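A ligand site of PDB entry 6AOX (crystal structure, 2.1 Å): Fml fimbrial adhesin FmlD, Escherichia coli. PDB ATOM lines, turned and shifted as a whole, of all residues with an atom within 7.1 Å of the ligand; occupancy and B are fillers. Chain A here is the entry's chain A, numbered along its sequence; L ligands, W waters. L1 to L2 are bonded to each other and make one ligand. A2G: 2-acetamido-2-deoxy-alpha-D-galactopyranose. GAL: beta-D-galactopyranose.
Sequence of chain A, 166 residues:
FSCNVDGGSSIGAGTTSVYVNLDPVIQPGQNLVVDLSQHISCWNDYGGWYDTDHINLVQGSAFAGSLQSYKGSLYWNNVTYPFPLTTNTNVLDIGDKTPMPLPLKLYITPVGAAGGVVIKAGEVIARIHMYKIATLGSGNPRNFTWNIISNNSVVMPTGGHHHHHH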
ATOM      1  N   PHE A   1      26.118 -11.225 -12.531  1.00  0.00           N
ATOM      2  CA  PHE A   1      25.919 -11.394 -14.003  1.00  0.00           C
ATOM      3  C   PHE A   1      24.471 -11.136 -14.378  1.00  0.00           C
ATOM      4  O   PHE A   1      23.548 -11.555 -13.669  1.00  0.00           O
ATOM      5  CB  PHE A   1      26.333 -12.799 -14.447  1.00  0.00           C
ATOM      6  CG  PHE A   1      26.132 -13.051 -15.912  1.00  0.00           C
ATOM      7  CD1 PHE A   1      25.080 -13.812 -16.365  1.00  0.00           C
ATOM      8  CD2 PHE A   1      27.007 -12.501 -16.838  1.00  0.00           C
ATOM      9  CE1 PHE A   1      24.896 -14.038 -17.720  1.00  0.00           C
ATOM     10  CE2 PHE A   1      26.838 -12.719 -18.188  1.00  0.00           C
ATOM     11  CZ  PHE A   1      25.777 -13.486 -18.627  1.00  0.00           C
ATOM     12  N   SER A   2      24.270 -10.455 -15.493  1.00  0.00           N
ATOM     13  CA  SER A   2      22.925 -10.065 -15.918  1.00  0.00           C
ATOM     14  C   SER A   2      22.739 -10.160 -17.422  1.00  0.00           C
ATOM     15  O   SER A   2      23.687 -10.023 -18.205  1.00  0.00           O
ATOM     16  CB  SER A   2      22.632  -8.639 -15.469  1.00  0.00           C
ATOM     17  OG  SER A   2      22.784  -8.500 -14.063  1.00  0.00           O
ATOM     18  N   GLY A  12      18.682 -12.293 -13.869  1.00  0.00           N
ATOM     19  CA  GLY A  12      19.813 -12.867 -13.140  1.00  0.00           C
ATOM     20  C   GLY A  12      19.841 -14.385 -13.197  1.00  0.00           C
ATOM     21  O   GLY A  12      20.865 -15.002 -12.929  1.00  0.00           O
ATOM     22  N   TRP A  43      25.889  -8.698 -19.725  1.00  0.00           N
ATOM     23  CA  TRP A  43      27.028  -7.908 -19.276  1.00  0.00           C
ATOM     24  C   TRP A  43      27.512  -8.355 -17.902  1.00  0.00           C
ATOM     25  O   TRP A  43      26.802  -9.058 -17.181  1.00  0.00           O
ATOM     26  CB  TRP A  43      26.664  -6.419 -19.224  1.00  0.00           C
ATOM     27  CG  TRP A  43      25.524  -6.104 -18.302  1.00  0.00           C
ATOM     28  CD1 TRP A  43      25.615  -5.645 -17.015  1.00  0.00           C
ATOM     29  CD2 TRP A  43      24.120  -6.219 -18.590  1.00  0.00           C
ATOM     30  NE1 TRP A  43      24.353  -5.463 -16.487  1.00  0.00           N
ATOM     31  CE2 TRP A  43      23.423  -5.809 -17.430  1.00  0.00           C
ATOM     32  CE3 TRP A  43      23.386  -6.625 -19.703  1.00  0.00           C
ATOM     33  CZ2 TRP A  43      22.036  -5.801 -17.357  1.00  0.00           C
ATOM     34  CZ3 TRP A  43      22.010  -6.611 -19.635  1.00  0.00           C
ATOM     35  CH2 TRP A  43      21.348  -6.208 -18.467  1.00  0.00           C
ATOM     36  N   ASN A  44      28.733  -7.950 -17.553  1.00  0.00           N
ATOM     37  CA  ASN A  44      29.264  -8.143 -16.218  1.00  0.00           C
ATOM     38  C   ASN A  44      28.748  -7.028 -15.312  1.00  0.00           C
ATOM     39  O   ASN A  44      28.673  -5.880 -15.747  1.00  0.00           O
ATOM     40  CB  ASN A  44      30.797  -8.161 -16.250  1.00  0.00           C
ATOM     41  CG  ASN A  44      31.410  -8.511 -14.914  1.00  0.00           C
ATOM     42  OD1 ASN A  44      31.290  -7.761 -13.942  1.00  0.00           O
ATOM     43  ND2 ASN A  44      32.085  -9.652 -14.856  1.00  0.00           N
ATOM     44  N   ASP A  45      28.409  -7.348 -14.076  1.00  0.00           N
ATOM     45  CA  ASP A  45      27.715  -6.384 -13.218  1.00  0.00           C
ATOM     46  C   ASP A  45      28.656  -5.437 -12.476  1.00  0.00           C
ATOM     47  O   ASP A  45      28.195  -4.432 -11.928  1.00  0.00           O
ATOM     48  CB  ASP A  45      26.837  -7.116 -12.201  1.00  0.00           C
ATOM     49  CG  ASP A  45      25.551  -7.633 -12.807  1.00  0.00           C
ATOM     50  OD1 ASP A  45      24.826  -6.845 -13.443  1.00  0.00           O
ATOM     51  OD2 ASP A  45      25.260  -8.835 -12.622  1.00  0.00           O
ATOM     52  N   TYR A  46      29.948  -5.739 -12.456  1.00  0.00           N
ATOM     53  CA  TYR A  46      30.924  -4.850 -11.810  1.00  0.00           C
ATOM     54  C   TYR A  46      31.828  -4.190 -12.842  1.00  0.00           C
ATOM     55  O   TYR A  46      32.109  -2.989 -12.753  1.00  0.00           O
ATOM     56  CB  TYR A  46      31.749  -5.614 -10.773  1.00  0.00           C
ATOM     57  CG  TYR A  46      30.944  -6.059  -9.570  1.00  0.00           C
ATOM     58  CD1 TYR A  46      30.250  -5.149  -8.783  1.00  0.00           C
ATOM     59  CD2 TYR A  46      30.892  -7.407  -9.210  1.00  0.00           C
ATOM     60  CE1 TYR A  46      29.511  -5.547  -7.685  1.00  0.00           C
ATOM     61  CE2 TYR A  46      30.164  -7.816  -8.104  1.00  0.00           C
ATOM     62  CZ  TYR A  46      29.476  -6.892  -7.343  1.00  0.00           C
ATOM     63  OH  TYR A  46      28.760  -7.317  -6.252  1.00  0.00           O
ATOM     64  N   GLY A  47      32.307  -4.971 -13.812  1.00  0.00           N
ATOM     65  CA  GLY A  47      33.091  -4.416 -14.897  1.00  0.00           C
ATOM     66  C   GLY A  47      34.597  -4.564 -14.704  1.00  0.00           C
ATOM     67  O   GLY A  47      35.052  -5.009 -13.654  1.00  0.00           O
ATOM     68  N   ASP A  51      35.577  -9.496 -11.763  1.00  0.00           N
ATOM     69  CA  ASP A  51      35.017 -10.800 -11.432  1.00  0.00           C
ATOM     70  C   ASP A  51      34.387 -11.357 -12.703  1.00  0.00           C
ATOM     71  O   ASP A  51      33.178 -11.245 -12.903  1.00  0.00           O
ATOM     72  CB  ASP A  51      34.014 -10.691 -10.290  1.00  0.00           C
ATOM     73  CG  ASP A  51      33.491 -12.047  -9.840  1.00  0.00           C
ATOM     74  OD1 ASP A  51      34.067 -13.076 -10.237  1.00  0.00           O
ATOM     75  OD2 ASP A  51      32.514 -12.071  -9.053  1.00  0.00           O
ATOM     76  N   THR A  52      35.220 -11.946 -13.548  1.00  0.00           N
ATOM     77  CA  THR A  52      34.805 -12.350 -14.884  1.00  0.00           C
ATOM     78  C   THR A  52      33.746 -13.451 -14.845  1.00  0.00           C
ATOM     79  O   THR A  52      33.866 -14.430 -14.107  1.00  0.00           O
ATOM     80  CB  THR A  52      36.014 -12.834 -15.712  1.00  0.00           C
ATOM     81  OG1 THR A  52      36.946 -11.761 -15.860  1.00  0.00           O
ATOM     82  CG2 THR A  52      35.566 -13.321 -17.094  1.00  0.00           C
ATOM     83  N   ASP A  53      32.709 -13.261 -15.647  1.00  0.00           N
ATOM     84  CA  ASP A  53      31.640 -14.232 -15.776  1.00  0.00           C
ATOM     85  C   ASP A  53      31.978 -15.212 -16.891  1.00  0.00           C
ATOM     86  O   ASP A  53      32.478 -14.817 -17.938  1.00  0.00           O
ATOM     87  CB  ASP A  53      30.319 -13.523 -16.084  1.00  0.00           C
ATOM     88  CG  ASP A  53      29.845 -12.668 -14.928  1.00  0.00           C
ATOM     89  OD1 ASP A  53      29.825 -13.171 -13.782  1.00  0.00           O
ATOM     90  OD2 ASP A  53      29.502 -11.486 -15.152  1.00  0.00           O
ATOM     91  N   ILE A  94      32.723 -12.796 -20.118  1.00  0.00           N
ATOM     92  CA  ILE A  94      32.099 -11.482 -20.133  1.00  0.00           C
ATOM     93  C   ILE A  94      32.512 -10.706 -18.889  1.00  0.00           C
ATOM     94  O   ILE A  94      32.261 -11.142 -17.765  1.00  0.00           O
ATOM     95  CB  ILE A  94      30.559 -11.607 -20.205  1.00  0.00           C
ATOM     96  CG1 ILE A  94      30.160 -12.227 -21.552  1.00  0.00           C
ATOM     97  CG2 ILE A  94      29.877 -10.249 -19.996  1.00  0.00           C
ATOM     98  CD1 ILE A  94      28.663 -12.322 -21.806  1.00  0.00           C
ATOM     99  N   LYS A  97      30.859  -3.847 -18.661  1.00  0.00           N
ATOM    100  CA  LYS A  97      29.548  -3.410 -18.188  1.00  0.00           C
ATOM    101  C   LYS A  97      28.606  -3.054 -19.331  1.00  0.00           C
ATOM    102  O   LYS A  97      27.397  -3.063 -19.154  1.00  0.00           O
ATOM    103  CB  LYS A  97      29.679  -2.200 -17.276  1.00  0.00           C
ATOM    104  CG  LYS A  97      29.468  -2.491 -15.812  1.00  0.00           C
ATOM    105  CD  LYS A  97      29.403  -1.181 -15.034  1.00  0.00           C
ATOM    106  CE  LYS A  97      28.577  -1.316 -13.771  1.00  0.00           C
ATOM    107  NZ  LYS A  97      28.440  -0.002 -13.073  1.00  0.00           N
ATOM    108  N   LYS A 132      25.986 -20.132 -16.134  1.00  0.00           N
ATOM    109  CA  LYS A 132      26.875 -19.060 -15.705  1.00  0.00           C
ATOM    110  C   LYS A 132      27.565 -19.429 -14.418  1.00  0.00           C
ATOM    111  O   LYS A 132      26.937 -19.939 -13.496  1.00  0.00           O
ATOM    112  CB  LYS A 132      26.094 -17.751 -15.507  1.00  0.00           C
ATOM    113  CG  LYS A 132      26.903 -16.629 -14.855  1.00  0.00           C
ATOM    114  CD  LYS A 132      26.567 -16.465 -13.377  1.00  0.00           C
ATOM    115  CE  LYS A 132      27.653 -15.674 -12.648  1.00  0.00           C
ATOM    116  NZ  LYS A 132      27.319 -15.423 -11.209  1.00  0.00           N
ATOM    117  N   ILE A 133      28.878 -19.218 -14.371  1.00  0.00           N
ATOM    118  CA  ILE A 133      29.620 -19.250 -13.120  1.00  0.00           C
ATOM    119  C   ILE A 133      30.731 -18.208 -13.239  1.00  0.00           C
ATOM    120  O   ILE A 133      31.332 -18.063 -14.307  1.00  0.00           O
ATOM    121  CB  ILE A 133      30.194 -20.645 -12.809  1.00  0.00           C
ATOM    122  CG1 ILE A 133      30.828 -20.664 -11.409  1.00  0.00           C
ATOM    123  CG2 ILE A 133      31.202 -21.076 -13.864  1.00  0.00           C
ATOM    124  CD1 ILE A 133      31.091 -22.064 -10.878  1.00  0.00           C
ATOM    125  N   ALA A 134      31.000 -17.496 -12.149  1.00  0.00           N
ATOM    126  CA  ALA A 134      31.960 -16.399 -12.181  1.00  0.00           C
ATOM    127  C   ALA A 134      33.332 -16.912 -11.757  1.00  0.00           C
ATOM    128  O   ALA A 134      33.591 -18.120 -11.799  1.00  0.00           O
ATOM    129  CB  ALA A 134      31.490 -15.258 -11.295  1.00  0.00           C
ATOM    130  N   THR A 135      34.210 -16.005 -11.331  1.00  0.00           N
ATOM    131  CA  THR A 135      35.602 -16.347 -11.036  1.00  0.00           C
ATOM    132  C   THR A 135      35.914 -16.256  -9.549  1.00  0.00           C
ATOM    133  O   THR A 135      36.565 -17.131  -8.974  1.00  0.00           O
ATOM    134  CB  THR A 135      36.566 -15.412 -11.789  1.00  0.00           C
ATOM    135  OG1 THR A 135      36.240 -15.400 -13.192  1.00  0.00           O
ATOM    136  CG2 THR A 135      38.014 -15.839 -11.596  1.00  0.00           C
ATOM    137  N   LEU A 136      35.446 -15.184  -8.928  1.00  0.00           N
ATOM    138  CA  LEU A 136      35.705 -14.926  -7.520  1.00  0.00           C
ATOM    139  C   LEU A 136      34.719 -15.660  -6.612  1.00  0.00           C
ATOM    140  O   LEU A 136      33.537 -15.799  -6.942  1.00  0.00           O
ATOM    141  CB  LEU A 136      35.675 -13.417  -7.278  1.00  0.00           C
ATOM    142  CG  LEU A 136      37.063 -12.756  -7.305  1.00  0.00           C
ATOM    143  CD1 LEU A 136      37.961 -13.248  -8.452  1.00  0.00           C
ATOM    144  CD2 LEU A 136      36.919 -11.246  -7.342  1.00  0.00           C
ATOM    145  N   SER A 138      32.635 -18.435  -4.877  1.00  0.00           N
ATOM    146  CA  SER A 138      32.035 -19.660  -5.387  1.00  0.00           C
ATOM    147  C   SER A 138      31.725 -19.509  -6.872  1.00  0.00           C
ATOM    148  O   SER A 138      31.549 -20.494  -7.590  1.00  0.00           O
ATOM    149  CB  SER A 138      30.756 -20.006  -4.619  1.00  0.00           C
ATOM    150  OG  SER A 138      29.853 -18.906  -4.594  1.00  0.00           O
ATOM    151  N   GLY A 139      31.665 -18.263  -7.320  1.00  0.00           N
ATOM    152  CA  GLY A 139      31.314 -17.932  -8.683  1.00  0.00           C
ATOM    153  C   GLY A 139      29.821 -17.717  -8.778  1.00  0.00           C
ATOM    154  O   GLY A 139      29.321 -17.222  -9.783  1.00  0.00           O
ATOM    155  N   ASN A 140      29.115 -18.063  -7.697  1.00  0.00           N
ATOM    156  CA  ASN A 140      27.657 -17.941  -7.616  1.00  0.00           C
ATOM    157  C   ASN A 140      26.998 -18.380  -8.918  1.00  0.00           C
ATOM    158  O   ASN A 140      26.432 -17.554  -9.641  1.00  0.00           O
ATOM    159  CB  ASN A 140      27.251 -16.513  -7.263  1.00  0.00           C
ATOM    160  CG  ASN A 140      27.741 -16.100  -5.882  1.00  0.00           C
ATOM    161  OD1 ASN A 140      28.021 -16.955  -5.033  1.00  0.00           O
ATOM    162  ND2 ASN A 140      27.828 -14.802  -5.648  1.00  0.00           N
ATOM    163  N   PRO A 141      27.102 -19.681  -9.237  1.00  0.00           N
ATOM    164  CA  PRO A 141      26.610 -20.171 -10.525  1.00  0.00           C
ATOM    165  C   PRO A 141      25.104 -19.959 -10.712  1.00  0.00           C
ATOM    166  O   PRO A 141      24.344 -20.115  -9.764  1.00  0.00           O
ATOM    167  CB  PRO A 141      26.962 -21.662 -10.486  1.00  0.00           C
ATOM    168  CG  PRO A 141      27.029 -21.998  -9.043  1.00  0.00           C
ATOM    169  CD  PRO A 141      27.578 -20.772  -8.372  1.00  0.00           C
ATOM    170  N   ARG A 142      24.714 -19.604 -11.932  1.00  0.00           N
ATOM    171  CA  ARG A 142      23.312 -19.382 -12.269  1.00  0.00           C
ATOM    172  C   ARG A 142      22.967 -20.110 -13.554  1.00  0.00           C
ATOM    173  O   ARG A 142      23.820 -20.327 -14.402  1.00  0.00           O
ATOM    174  CB  ARG A 142      23.023 -17.890 -12.441  1.00  0.00           C
ATOM    175  CG  ARG A 142      23.349 -17.016 -11.245  1.00  0.00           C
ATOM    176  CD  ARG A 142      22.345 -17.194 -10.124  1.00  0.00           C
ATOM    177  NE  ARG A 142      22.558 -16.218  -9.054  1.00  0.00           N
ATOM    178  CZ  ARG A 142      22.034 -15.000  -9.047  1.00  0.00           C
ATOM    179  NH1 ARG A 142      21.266 -14.580 -10.048  1.00  0.00           N
ATOM    180  NH2 ARG A 142      22.277 -14.179  -8.031  1.00  0.00           N
HETATM  181  O5  A2G L   1      24.528  -6.699  -7.204  1.00  0.00           O
HETATM  182  C1  A2G L   1      24.516  -7.838  -6.380  1.00  0.00           C
HETATM  183  O1  A2G L   1      25.490  -7.702  -5.373  1.00  0.00           O
HETATM  184  C2  A2G L   1      24.813  -9.097  -7.177  1.00  0.00           C
HETATM  185  N2  A2G L   1      24.980 -10.185  -6.276  1.00  0.00           N
HETATM  186  C3  A2G L   1      26.084  -8.924  -7.994  1.00  0.00           C
HETATM  187  O3  A2G L   1      26.205 -10.024  -8.863  1.00  0.00           O
HETATM  188  C4  A2G L   1      26.003  -7.665  -8.812  1.00  0.00           C
HETATM  189  O4  A2G L   1      24.949  -7.788  -9.745  1.00  0.00           O
HETATM  190  C5  A2G L   1      25.737  -6.487  -7.891  1.00  0.00           C
HETATM  191  C6  A2G L   1      25.641  -5.213  -8.705  1.00  0.00           C
HETATM  192  O6  A2G L   1      25.450  -4.116  -7.840  1.00  0.00           O
HETATM  193  C7  A2G L   1      24.460 -11.467  -6.577  1.00  0.00           C
HETATM  194  O7  A2G L   1      23.870 -11.656  -7.613  1.00  0.00           O
HETATM  195  C8  A2G L   1      24.653 -12.623  -5.606  1.00  0.00           C
HETATM  196  C1  GAL L   2      27.546 -10.432  -9.070  1.00  0.00           C
HETATM  197  C2  GAL L   2      27.585 -11.943  -9.014  1.00  0.00           C
HETATM  198  C3  GAL L   2      28.979 -12.437  -9.333  1.00  0.00           C
HETATM  199  C4  GAL L   2      29.376 -11.911 -10.683  1.00  0.00           C
HETATM  200  C5  GAL L   2      29.291 -10.395 -10.657  1.00  0.00           C
HETATM  201  C6  GAL L   2      29.693  -9.851 -12.010  1.00  0.00           C
HETATM  202  O2  GAL L   2      27.231 -12.351  -7.712  1.00  0.00           O
HETATM  203  O3  GAL L   2      28.998 -13.847  -9.330  1.00  0.00           O
HETATM  204  O4  GAL L   2      28.486 -12.400 -11.663  1.00  0.00           O
HETATM  205  O5  GAL L   2      27.977  -9.996 -10.341  1.00  0.00           O
HETATM  206  O6  GAL L   2      28.700 -10.172 -12.963  1.00  0.00           O
HETATM  207  O   HOH W   1      31.819 -14.316  -8.253  1.00  0.00           O
HETATM  208  O   HOH W   2      25.126 -13.230 -11.179  1.00  0.00           O
HETATM  209  O   HOH W   3      24.848  -4.372  -5.050  1.00  0.00           O
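The backbone NH (N) of Phe 1 lies within hydrogen-bond range of an oxygen (O4) of GAL L2, 2.8 Å away. The side-chain amide nitrogen of Asn 140 sits at hydrogen-bond distance from an oxygen (O2) of GAL L2 (3.3 Å). The backbone carbonyl oxygen of Gly 139 is in hydrogen-bond range of an oxygen (O3) of GAL L2, 3.4 Å away. NH2 of Arg 142 sits at hydrogen-bond distance from O7 of A2G L1 (3.0 Å). The side-chain carboxylate (OD2) of Asp 45 is in hydrogen-bond range of an oxygen (O4) of A2G L1 (3.1 Å). The backbone NH of Asp 45 lies within hydrogen-bond range of an oxygen (O6) of GAL L2, at 3.0 Å. An oxygen (O3) of GAL L2 is in hydrogen-bond range of the side-chain amino group of Lys 132. O1 of A2G L1 is in hydrogen-bond range of OH of Tyr 46, 3.4 Å away. O4 of GAL L2 lies within hydrogen-bond range of OD1 of Asp 53 (2.6 Å).
The backbone carbonyl oxygen of Ile 94 lies within hydrogen-bond range of the side-chain amide nitrogen of Asn 44, 3.3 Å away. OD1 of Asn 44 is in hydrogen-bond range of N of Tyr 46 (2.8 Å). The side-chain carboxylate (OD1) of Asp 45 is in hydrogen-bond range of the indole nitrogen (NE1) of Trp 43 (3.4 Å). The side-chain amino group (NZ) of Lys 132 is in hydrogen-bond range of the backbone carbonyl oxygen (O) of Gly 139. OD1 of Asp 51 lies within hydrogen-bond range of N of Thr 135. The side-chain carboxylate of Asp 53 sits at hydrogen-bond distance from the side-chain amide nitrogen of Asn 44 (3.2 Å). The backbone carbonyl oxygen (O) of Gly 12 is in hydrogen-bond range of the guanidinium group (NH1) of Arg 142 (2.9 Å). The backbone carbonyl oxygen (O) of Asp 53 is in hydrogen-bond range of the backbone NH (N) of Ile 94, at 3.0 Å.
OD1 of Asn 44 touches C6 of GAL L2, at 3.3 Å. OD2 of Asp 51 touches C4 of GAL L2 (3.5 Å). CB of Ala 134 touches O3 of GAL L2, at 3.5 Å. Hydrophobic or aromatic side chains that line the ligand: Phe 1, Tyr 46 and Ala 134.
Water W1 lies within hydrogen-bond range of the side-chain carboxylate of Asp 51 (2.5 Å), the backbone carbonyl oxygen of Leu 136 (2.6 Å) and an oxygen (O3) of GAL L2 (3.1 Å). Water W2 lies within hydrogen-bond range of the backbone NH (N) of Phe 1 (2.6 Å), the side-chain amino group (NZ) of Lys 132 (3.1 Å) and an oxygen (O4) of GAL L2 (3.5 Å).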
